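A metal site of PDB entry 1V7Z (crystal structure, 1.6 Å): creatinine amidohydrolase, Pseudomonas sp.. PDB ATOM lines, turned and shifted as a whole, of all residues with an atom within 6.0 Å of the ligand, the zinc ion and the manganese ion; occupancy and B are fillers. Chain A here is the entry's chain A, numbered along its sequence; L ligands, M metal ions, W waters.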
ATOM      1  N   ALA A  32     -26.360  -6.557 -21.405  1.00  0.00           N
ATOM      2  CA  ALA A  32     -26.148  -6.482 -19.963  1.00  0.00           C
ATOM      3  C   ALA A  32     -26.935  -5.314 -19.406  1.00  0.00           C
ATOM      4  O   ALA A  32     -27.325  -4.413 -20.148  1.00  0.00           O
ATOM      5  CB  ALA A  32     -24.672  -6.291 -19.642  1.00  0.00           C
ATOM      6  N   GLU A  34     -25.869  -2.694 -16.696  1.00  0.00           N
ATOM      7  CA  GLU A  34     -24.564  -2.369 -16.142  1.00  0.00           C
ATOM      8  C   GLU A  34     -24.401  -0.863 -16.040  1.00  0.00           C
ATOM      9  O   GLU A  34     -24.766  -0.126 -16.953  1.00  0.00           O
ATOM     10  CB  GLU A  34     -23.478  -2.920 -17.053  1.00  0.00           C
ATOM     11  CG  GLU A  34     -22.058  -2.739 -16.548  1.00  0.00           C
ATOM     12  CD  GLU A  34     -21.018  -3.167 -17.564  1.00  0.00           C
ATOM     13  OE1 GLU A  34     -19.958  -3.681 -17.173  1.00  0.00           O
ATOM     14  OE2 GLU A  34     -21.266  -2.997 -18.780  1.00  0.00           O
ATOM     15  N   HIS A  36     -22.986   2.702 -16.387  1.00  0.00           N
ATOM     16  CA  HIS A  36     -22.235   3.357 -17.454  1.00  0.00           C
ATOM     17  C   HIS A  36     -21.977   4.832 -17.111  1.00  0.00           C
ATOM     18  O   HIS A  36     -22.230   5.720 -17.909  1.00  0.00           O
ATOM     19  CB  HIS A  36     -22.994   3.239 -18.769  1.00  0.00           C
ATOM     20  CG  HIS A  36     -22.772   1.932 -19.480  1.00  0.00           C
ATOM     21  ND1 HIS A  36     -23.523   0.806 -19.225  1.00  0.00           N
ATOM     22  CD2 HIS A  36     -21.888   1.589 -20.437  1.00  0.00           C
ATOM     23  CE1 HIS A  36     -23.115  -0.184 -20.002  1.00  0.00           C
ATOM     24  NE2 HIS A  36     -22.117   0.271 -20.754  1.00  0.00           N
ATOM     25  N   VAL A  44     -27.422   0.324 -21.977  1.00  0.00           N
ATOM     26  CA  VAL A  44     -26.616   0.595 -23.178  1.00  0.00           C
ATOM     27  C   VAL A  44     -26.220  -0.667 -23.937  1.00  0.00           C
ATOM     28  O   VAL A  44     -26.337  -0.728 -25.155  1.00  0.00           O
ATOM     29  CB  VAL A  44     -25.319   1.389 -22.832  1.00  0.00           C
ATOM     30  CG1 VAL A  44     -24.349   1.422 -24.013  1.00  0.00           C
ATOM     31  CG2 VAL A  44     -25.652   2.813 -22.407  1.00  0.00           C
ATOM     32  N   ASP A  45     -25.762  -1.690 -23.217  1.00  0.00           N
ATOM     33  CA  ASP A  45     -25.228  -2.893 -23.845  1.00  0.00           C
ATOM     34  C   ASP A  45     -26.287  -3.766 -24.534  1.00  0.00           C
ATOM     35  O   ASP A  45     -25.942  -4.661 -25.310  1.00  0.00           O
ATOM     36  CB  ASP A  45     -24.476  -3.744 -22.817  1.00  0.00           C
ATOM     37  CG  ASP A  45     -23.175  -3.106 -22.361  1.00  0.00           C
ATOM     38  OD1 ASP A  45     -22.847  -1.957 -22.792  1.00  0.00           O
ATOM     39  OD2 ASP A  45     -22.407  -3.691 -21.563  1.00  0.00           O
ATOM     40  N   SER A  78     -12.506  -4.016 -17.549  1.00  0.00           N
ATOM     41  CA  SER A  78     -13.308  -3.811 -18.753  1.00  0.00           C
ATOM     42  C   SER A  78     -14.658  -3.111 -18.537  1.00  0.00           C
ATOM     43  O   SER A  78     -15.226  -2.594 -19.479  1.00  0.00           O
ATOM     44  CB  SER A  78     -13.529  -5.142 -19.494  1.00  0.00           C
ATOM     45  OG  SER A  78     -13.969  -6.167 -18.612  1.00  0.00           O
ATOM     46  N   GLY A  79     -15.191  -3.128 -17.326  1.00  0.00           N
ATOM     47  CA  GLY A  79     -16.521  -2.601 -17.061  1.00  0.00           C
ATOM     48  C   GLY A  79     -16.689  -1.916 -15.715  1.00  0.00           C
ATOM     49  O   GLY A  79     -17.811  -1.616 -15.323  1.00  0.00           O
ATOM     50  N   GLY A 119     -22.790  -7.195 -27.049  1.00  0.00           N
ATOM     51  CA  GLY A 119     -22.633  -5.791 -26.713  1.00  0.00           C
ATOM     52  C   GLY A 119     -22.003  -5.514 -25.360  1.00  0.00           C
ATOM     53  O   GLY A 119     -21.840  -4.361 -24.992  1.00  0.00           O
ATOM     54  N   HIS A 120     -21.616  -6.572 -24.631  1.00  0.00           N
ATOM     55  CA  HIS A 120     -21.008  -6.444 -23.312  1.00  0.00           C
ATOM     56  C   HIS A 120     -19.752  -7.301 -23.299  1.00  0.00           C
ATOM     57  O   HIS A 120     -19.797  -8.522 -23.477  1.00  0.00           O
ATOM     58  CB  HIS A 120     -22.011  -6.904 -22.269  1.00  0.00           C
ATOM     59  CG  HIS A 120     -21.483  -7.002 -20.865  1.00  0.00           C
ATOM     60  ND1 HIS A 120     -21.231  -5.906 -20.067  1.00  0.00           N
ATOM     61  CD2 HIS A 120     -21.262  -8.096 -20.097  1.00  0.00           C
ATOM     62  CE1 HIS A 120     -20.856  -6.329 -18.867  1.00  0.00           C
ATOM     63  NE2 HIS A 120     -20.889  -7.647 -18.850  1.00  0.00           N
ATOM     64  N   TYR A 121     -18.611  -6.635 -23.131  1.00  0.00           N
ATOM     65  CA  TYR A 121     -17.295  -7.220 -23.301  1.00  0.00           C
ATOM     66  C   TYR A 121     -17.135  -8.570 -22.599  1.00  0.00           C
ATOM     67  O   TYR A 121     -16.638  -9.538 -23.173  1.00  0.00           O
ATOM     68  CB  TYR A 121     -16.255  -6.238 -22.767  1.00  0.00           C
ATOM     69  CG  TYR A 121     -14.847  -6.544 -23.159  1.00  0.00           C
ATOM     70  CD1 TYR A 121     -14.284  -5.955 -24.292  1.00  0.00           C
ATOM     71  CD2 TYR A 121     -14.056  -7.396 -22.399  1.00  0.00           C
ATOM     72  CE1 TYR A 121     -12.982  -6.215 -24.661  1.00  0.00           C
ATOM     73  CE2 TYR A 121     -12.748  -7.662 -22.758  1.00  0.00           C
ATOM     74  CZ  TYR A 121     -12.213  -7.075 -23.895  1.00  0.00           C
ATOM     75  OH  TYR A 121     -10.919  -7.328 -24.254  1.00  0.00           O
ATOM     76  N   GLU A 122     -17.624  -8.627 -21.367  1.00  0.00           N
ATOM     77  CA  GLU A 122     -17.424  -9.786 -20.504  1.00  0.00           C
ATOM     78  C   GLU A 122     -18.212 -11.034 -20.909  1.00  0.00           C
ATOM     79  O   GLU A 122     -17.946 -12.121 -20.408  1.00  0.00           O
ATOM     80  CB  GLU A 122     -17.818  -9.402 -19.066  1.00  0.00           C
ATOM     81  CG  GLU A 122     -16.875  -8.447 -18.353  1.00  0.00           C
ATOM     82  CD  GLU A 122     -17.140  -6.965 -18.603  1.00  0.00           C
ATOM     83  OE1 GLU A 122     -17.862  -6.594 -19.543  1.00  0.00           O
ATOM     84  OE2 GLU A 122     -16.587  -6.150 -17.833  1.00  0.00           O
ATOM     85  N   TYR A 153     -19.712  -6.042 -31.664  1.00  0.00           N
ATOM     86  CA  TYR A 153     -19.935  -5.122 -32.799  1.00  0.00           C
ATOM     87  C   TYR A 153     -18.822  -4.094 -32.980  1.00  0.00           C
ATOM     88  O   TYR A 153     -18.502  -3.708 -34.116  1.00  0.00           O
ATOM     89  CB  TYR A 153     -21.335  -4.473 -32.744  1.00  0.00           C
ATOM     90  CG  TYR A 153     -21.498  -3.488 -31.618  1.00  0.00           C
ATOM     91  CD1 TYR A 153     -21.268  -2.135 -31.822  1.00  0.00           C
ATOM     92  CD2 TYR A 153     -21.867  -3.908 -30.349  1.00  0.00           C
ATOM     93  CE1 TYR A 153     -21.392  -1.233 -30.798  1.00  0.00           C
ATOM     94  CE2 TYR A 153     -21.985  -3.013 -29.315  1.00  0.00           C
ATOM     95  CZ  TYR A 153     -21.752  -1.673 -29.530  1.00  0.00           C
ATOM     96  OH  TYR A 153     -21.870  -0.778 -28.496  1.00  0.00           O
ATOM     97  N   TRP A 154     -18.202  -3.659 -31.879  1.00  0.00           N
ATOM     98  CA  TRP A 154     -17.083  -2.709 -31.944  1.00  0.00           C
ATOM     99  C   TRP A 154     -15.855  -3.211 -32.694  1.00  0.00           C
ATOM    100  O   TRP A 154     -15.080  -2.406 -33.202  1.00  0.00           O
ATOM    101  CB  TRP A 154     -16.664  -2.246 -30.541  1.00  0.00           C
ATOM    102  CG  TRP A 154     -16.387  -3.371 -29.566  1.00  0.00           C
ATOM    103  CD1 TRP A 154     -15.249  -4.115 -29.466  1.00  0.00           C
ATOM    104  CD2 TRP A 154     -17.278  -3.856 -28.552  1.00  0.00           C
ATOM    105  NE1 TRP A 154     -15.381  -5.039 -28.462  1.00  0.00           N
ATOM    106  CE2 TRP A 154     -16.614  -4.903 -27.882  1.00  0.00           C
ATOM    107  CE3 TRP A 154     -18.575  -3.513 -28.156  1.00  0.00           C
ATOM    108  CZ2 TRP A 154     -17.194  -5.608 -26.830  1.00  0.00           C
ATOM    109  CZ3 TRP A 154     -19.156  -4.219 -27.104  1.00  0.00           C
ATOM    110  CH2 TRP A 154     -18.461  -5.247 -26.459  1.00  0.00           C
ATOM    111  N   TRP A 174     -10.324  -1.812 -26.734  1.00  0.00           N
ATOM    112  CA  TRP A 174     -11.762  -1.930 -26.510  1.00  0.00           C
ATOM    113  C   TRP A 174     -12.115  -2.276 -25.052  1.00  0.00           C
ATOM    114  O   TRP A 174     -13.219  -1.999 -24.619  1.00  0.00           O
ATOM    115  CB  TRP A 174     -12.378  -2.950 -27.473  1.00  0.00           C
ATOM    116  CG  TRP A 174     -12.333  -2.515 -28.918  1.00  0.00           C
ATOM    117  CD1 TRP A 174     -11.752  -3.182 -29.954  1.00  0.00           C
ATOM    118  CD2 TRP A 174     -12.885  -1.318 -29.474  1.00  0.00           C
ATOM    119  NE1 TRP A 174     -11.913  -2.482 -31.129  1.00  0.00           N
ATOM    120  CE2 TRP A 174     -12.608  -1.330 -30.867  1.00  0.00           C
ATOM    121  CE3 TRP A 174     -13.592  -0.228 -28.945  1.00  0.00           C
ATOM    122  CZ2 TRP A 174     -13.007  -0.294 -31.720  1.00  0.00           C
ATOM    123  CZ3 TRP A 174     -13.998   0.787 -29.801  1.00  0.00           C
ATOM    124  CH2 TRP A 174     -13.692   0.747 -31.172  1.00  0.00           C
ATOM    125  N   ASP A 175     -11.169  -2.858 -24.315  1.00  0.00           N
ATOM    126  CA  ASP A 175     -11.361  -3.127 -22.873  1.00  0.00           C
ATOM    127  C   ASP A 175     -11.676  -1.888 -22.006  1.00  0.00           C
ATOM    128  O   ASP A 175     -12.623  -1.899 -21.225  1.00  0.00           O
ATOM    129  CB  ASP A 175     -10.165  -3.900 -22.274  1.00  0.00           C
ATOM    130  CG  ASP A 175      -8.824  -3.257 -22.590  1.00  0.00           C
ATOM    131  OD1 ASP A 175      -8.136  -2.843 -21.635  1.00  0.00           O
ATOM    132  OD2 ASP A 175      -8.391  -3.124 -23.753  1.00  0.00           O
ATOM    133  N   ILE A 176     -10.901  -0.804 -22.130  1.00  0.00           N
ATOM    134  CA  ILE A 176     -11.197   0.392 -21.335  1.00  0.00           C
ATOM    135  C   ILE A 176     -12.234   1.317 -21.986  1.00  0.00           C
ATOM    136  O   ILE A 176     -12.496   2.414 -21.487  1.00  0.00           O
ATOM    137  CB  ILE A 176      -9.904   1.154 -20.941  1.00  0.00           C
ATOM    138  CG1 ILE A 176      -9.150   1.637 -22.183  1.00  0.00           C
ATOM    139  CG2 ILE A 176      -9.023   0.275 -20.083  1.00  0.00           C
ATOM    140  CD1 ILE A 176      -8.362   2.909 -21.917  1.00  0.00           C
ATOM    141  N   GLU A 177     -12.846   0.846 -23.069  1.00  0.00           N
ATOM    142  CA  GLU A 177     -13.893   1.572 -23.755  1.00  0.00           C
ATOM    143  C   GLU A 177     -15.245   1.317 -23.088  1.00  0.00           C
ATOM    144  O   GLU A 177     -16.211   0.874 -23.724  1.00  0.00           O
ATOM    145  CB  GLU A 177     -13.936   1.172 -25.234  1.00  0.00           C
ATOM    146  CG  GLU A 177     -14.614   2.176 -26.131  1.00  0.00           C
ATOM    147  CD  GLU A 177     -14.276   3.606 -25.772  1.00  0.00           C
ATOM    148  OE1 GLU A 177     -13.101   4.005 -25.924  1.00  0.00           O
ATOM    149  OE2 GLU A 177     -15.172   4.323 -25.302  1.00  0.00           O
ATOM    150  N   HIS A 178     -15.321   1.601 -21.803  1.00  0.00           N
ATOM    151  CA  HIS A 178     -16.560   1.434 -21.056  1.00  0.00           C
ATOM    152  C   HIS A 178     -17.119   2.794 -20.671  1.00  0.00           C
ATOM    153  O   HIS A 178     -16.575   3.466 -19.803  1.00  0.00           O
ATOM    154  CB  HIS A 178     -16.333   0.586 -19.814  1.00  0.00           C
ATOM    155  CG  HIS A 178     -17.580   0.380 -19.030  1.00  0.00           C
ATOM    156  ND1 HIS A 178     -18.689  -0.252 -19.555  1.00  0.00           N
ATOM    157  CD2 HIS A 178     -17.938   0.780 -17.788  1.00  0.00           C
ATOM    158  CE1 HIS A 178     -19.663  -0.244 -18.674  1.00  0.00           C
ATOM    159  NE2 HIS A 178     -19.233   0.384 -17.589  1.00  0.00           N
ATOM    160  N   GLY A 179     -18.212   3.181 -21.319  1.00  0.00           N
ATOM    161  CA  GLY A 179     -18.857   4.450 -21.061  1.00  0.00           C
ATOM    162  C   GLY A 179     -18.077   5.641 -21.600  1.00  0.00           C
ATOM    163  O   GLY A 179     -18.310   6.768 -21.187  1.00  0.00           O
ATOM    164  N   PHE A 182     -16.814   5.888 -27.495  1.00  0.00           N
ATOM    165  CA  PHE A 182     -17.470   4.993 -28.444  1.00  0.00           C
ATOM    166  C   PHE A 182     -18.957   4.808 -28.129  1.00  0.00           C
ATOM    167  O   PHE A 182     -19.823   5.096 -28.950  1.00  0.00           O
ATOM    168  CB  PHE A 182     -16.756   3.632 -28.438  1.00  0.00           C
ATOM    169  CG  PHE A 182     -17.331   2.645 -29.415  1.00  0.00           C
ATOM    170  CD1 PHE A 182     -18.287   1.734 -29.005  1.00  0.00           C
ATOM    171  CD2 PHE A 182     -16.903   2.611 -30.742  1.00  0.00           C
ATOM    172  CE1 PHE A 182     -18.820   0.815 -29.891  1.00  0.00           C
ATOM    173  CE2 PHE A 182     -17.442   1.685 -31.629  1.00  0.00           C
ATOM    174  CZ  PHE A 182     -18.401   0.786 -31.199  1.00  0.00           C
ATOM    175  N   GLU A 183     -19.242   4.328 -26.926  1.00  0.00           N
ATOM    176  CA  GLU A 183     -20.629   4.047 -26.557  1.00  0.00           C
ATOM    177  C   GLU A 183     -21.430   5.328 -26.437  1.00  0.00           C
ATOM    178  O   GLU A 183     -22.575   5.376 -26.864  1.00  0.00           O
ATOM    179  CB  GLU A 183     -20.703   3.284 -25.231  1.00  0.00           C
ATOM    180  CG  GLU A 183     -20.260   1.834 -25.363  1.00  0.00           C
ATOM    181  CD  GLU A 183     -20.422   1.058 -24.068  1.00  0.00           C
ATOM    182  OE1 GLU A 183     -21.033  -0.015 -24.127  1.00  0.00           O
ATOM    183  OE2 GLU A 183     -19.932   1.508 -23.020  1.00  0.00           O
ATOM    184  N   LEU A 227     -14.268   3.886 -17.617  1.00  0.00           N
ATOM    185  CA  LEU A 227     -12.842   3.569 -17.724  1.00  0.00           C
ATOM    186  C   LEU A 227     -12.121   4.566 -18.627  1.00  0.00           C
ATOM    187  O   LEU A 227     -10.903   4.592 -18.681  1.00  0.00           O
ATOM    188  CB  LEU A 227     -12.650   2.132 -18.226  1.00  0.00           C
ATOM    189  CG  LEU A 227     -13.125   1.041 -17.242  1.00  0.00           C
ATOM    190  CD1 LEU A 227     -12.830  -0.343 -17.789  1.00  0.00           C
ATOM    191  CD2 LEU A 227     -12.498   1.208 -15.858  1.00  0.00           C
HETATM  192  O1  LIG L   1     -19.228  -3.881 -22.525  1.00  0.00           O
HETATM  193  C1  LIG L   1     -19.284  -2.637 -22.588  1.00  0.00           C
HETATM  194  O2  LIG L   1     -19.923  -1.954 -21.739  1.00  0.00           O
HETATM  195  C2  LIG L   1     -18.528  -1.914 -23.690  1.00  0.00           C
HETATM  196  N1  LIG L   1     -17.094  -2.249 -23.737  1.00  0.00           N
HETATM  197  C3  LIG L   1     -16.516  -2.341 -25.083  1.00  0.00           C
HETATM  198  C4  LIG L   1     -16.352  -2.437 -22.640  1.00  0.00           C
HETATM  199  N2  LIG L   1     -15.119  -2.685 -22.733  1.00  0.00           N
HETATM  200  N3  LIG L   1     -16.893  -2.356 -21.412  1.00  0.00           N
HETATM  201 ZN    ZN M   1     -21.352  -0.760 -22.302  1.00  0.00          ZN
HETATM  202 MN    MN M   2     -20.602  -3.790 -20.583  1.00  0.00          MN
HETATM  203  O   HOH W   1     -18.584  -4.039 -19.570  1.00  0.00           O
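Within 4 Å of the manganese ion: Glu 34, Asp 45 and His 120.
The backbone carbonyl oxygen (O) of Ser 78 is in hydrogen-bond range of a nitrogen (N3) of the ligand (2.6 Å). O of Trp 174 sits at hydrogen-bond distance from N2 of the ligand (2.8 Å). N of Tyr 121 lies close to O1 of the ligand (2.9 Å). The backbone carbonyl oxygen of Asp 175 is in hydrogen-bond range of a nitrogen (N2) of the ligand, at 3.0 Å. A nitrogen (N3) of the ligand sits at hydrogen-bond distance from a ring nitrogen (ND1) of His 178, 3.3 Å away.
The manganese ion is bound by OD2 of Asp 45 (2.1 Å), OE2 of Glu 34 (2.1 Å), ND1 of His 120 (2.3 Å), water W1 (2.3 Å), O2 of the ligand (2.3 Å) and O1 of the ligand (2.4 Å). The manganese ion has six donor atoms within binding distance.
Water W1 lies within hydrogen-bond range of the side-chain carboxylate of Glu 122, the side-chain carboxylate of Glu 34 and a nitrogen (N3) of the ligand.
OE2 of Glu 183 lies within hydrogen-bond range of N of Gly 179. A ring nitrogen (ND1) of His 36 lies within hydrogen-bond range of the backbone carbonyl oxygen (O) of Glu 34 (2.8 Å). The side-chain carboxylate of Glu 122 lies close to a ring nitrogen (NE2) of His 120 (3.3 Å). OE2 of Glu 122 sits at hydrogen-bond distance from OG of Ser 78 (2.7 Å). A ring nitrogen (NE2) of His 178 is in hydrogen-bond range of the backbone carbonyl oxygen (O) of Gly 79. O of His 178 sits at hydrogen-bond distance from N of Leu 227, at 3.2 Å. The side-chain carboxylate of Glu 177 sits at hydrogen-bond distance from the backbone NH of Phe 182 (3.2 Å).
Merely in contact with the zinc ion: His 178 (3.9 Å). Four residues have an atom within 4 Å of the zinc ion: His 36, Asp 45, His 178 and Glu 183. The nearest printed residue that does not touch the zinc ion is Val 44 (4.1 Å).
The zinc ion is bound by O2 of the ligand (1.9 Å), OD1 of Asp 45 (2.0 Å), OE1 of Glu 183 (2.0 Å) and NE2 of His 36 (2.0 Å). Slightly farther from the zinc ion lies the side-chain carboxylate (OE2) of Glu 183 (2.8 Å).
O of Glu 177 lies close to N1 of the ligand, 3.2 Å away. Residues that only touch the ligand: Gly 119 (3.6 Å) and Trp 154 (3.8 Å). Hydrophobic or aromatic side chains that line the ligand: Tyr 121, Trp 154 and His 178. Within 4 Å of the ligand: Glu 34, His 36, Asp 45, Ser 78, Gly 119, His 120, Tyr 121, Trp 154, Trp 174, Asp 175, Glu 177, His 178 and Glu 183.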
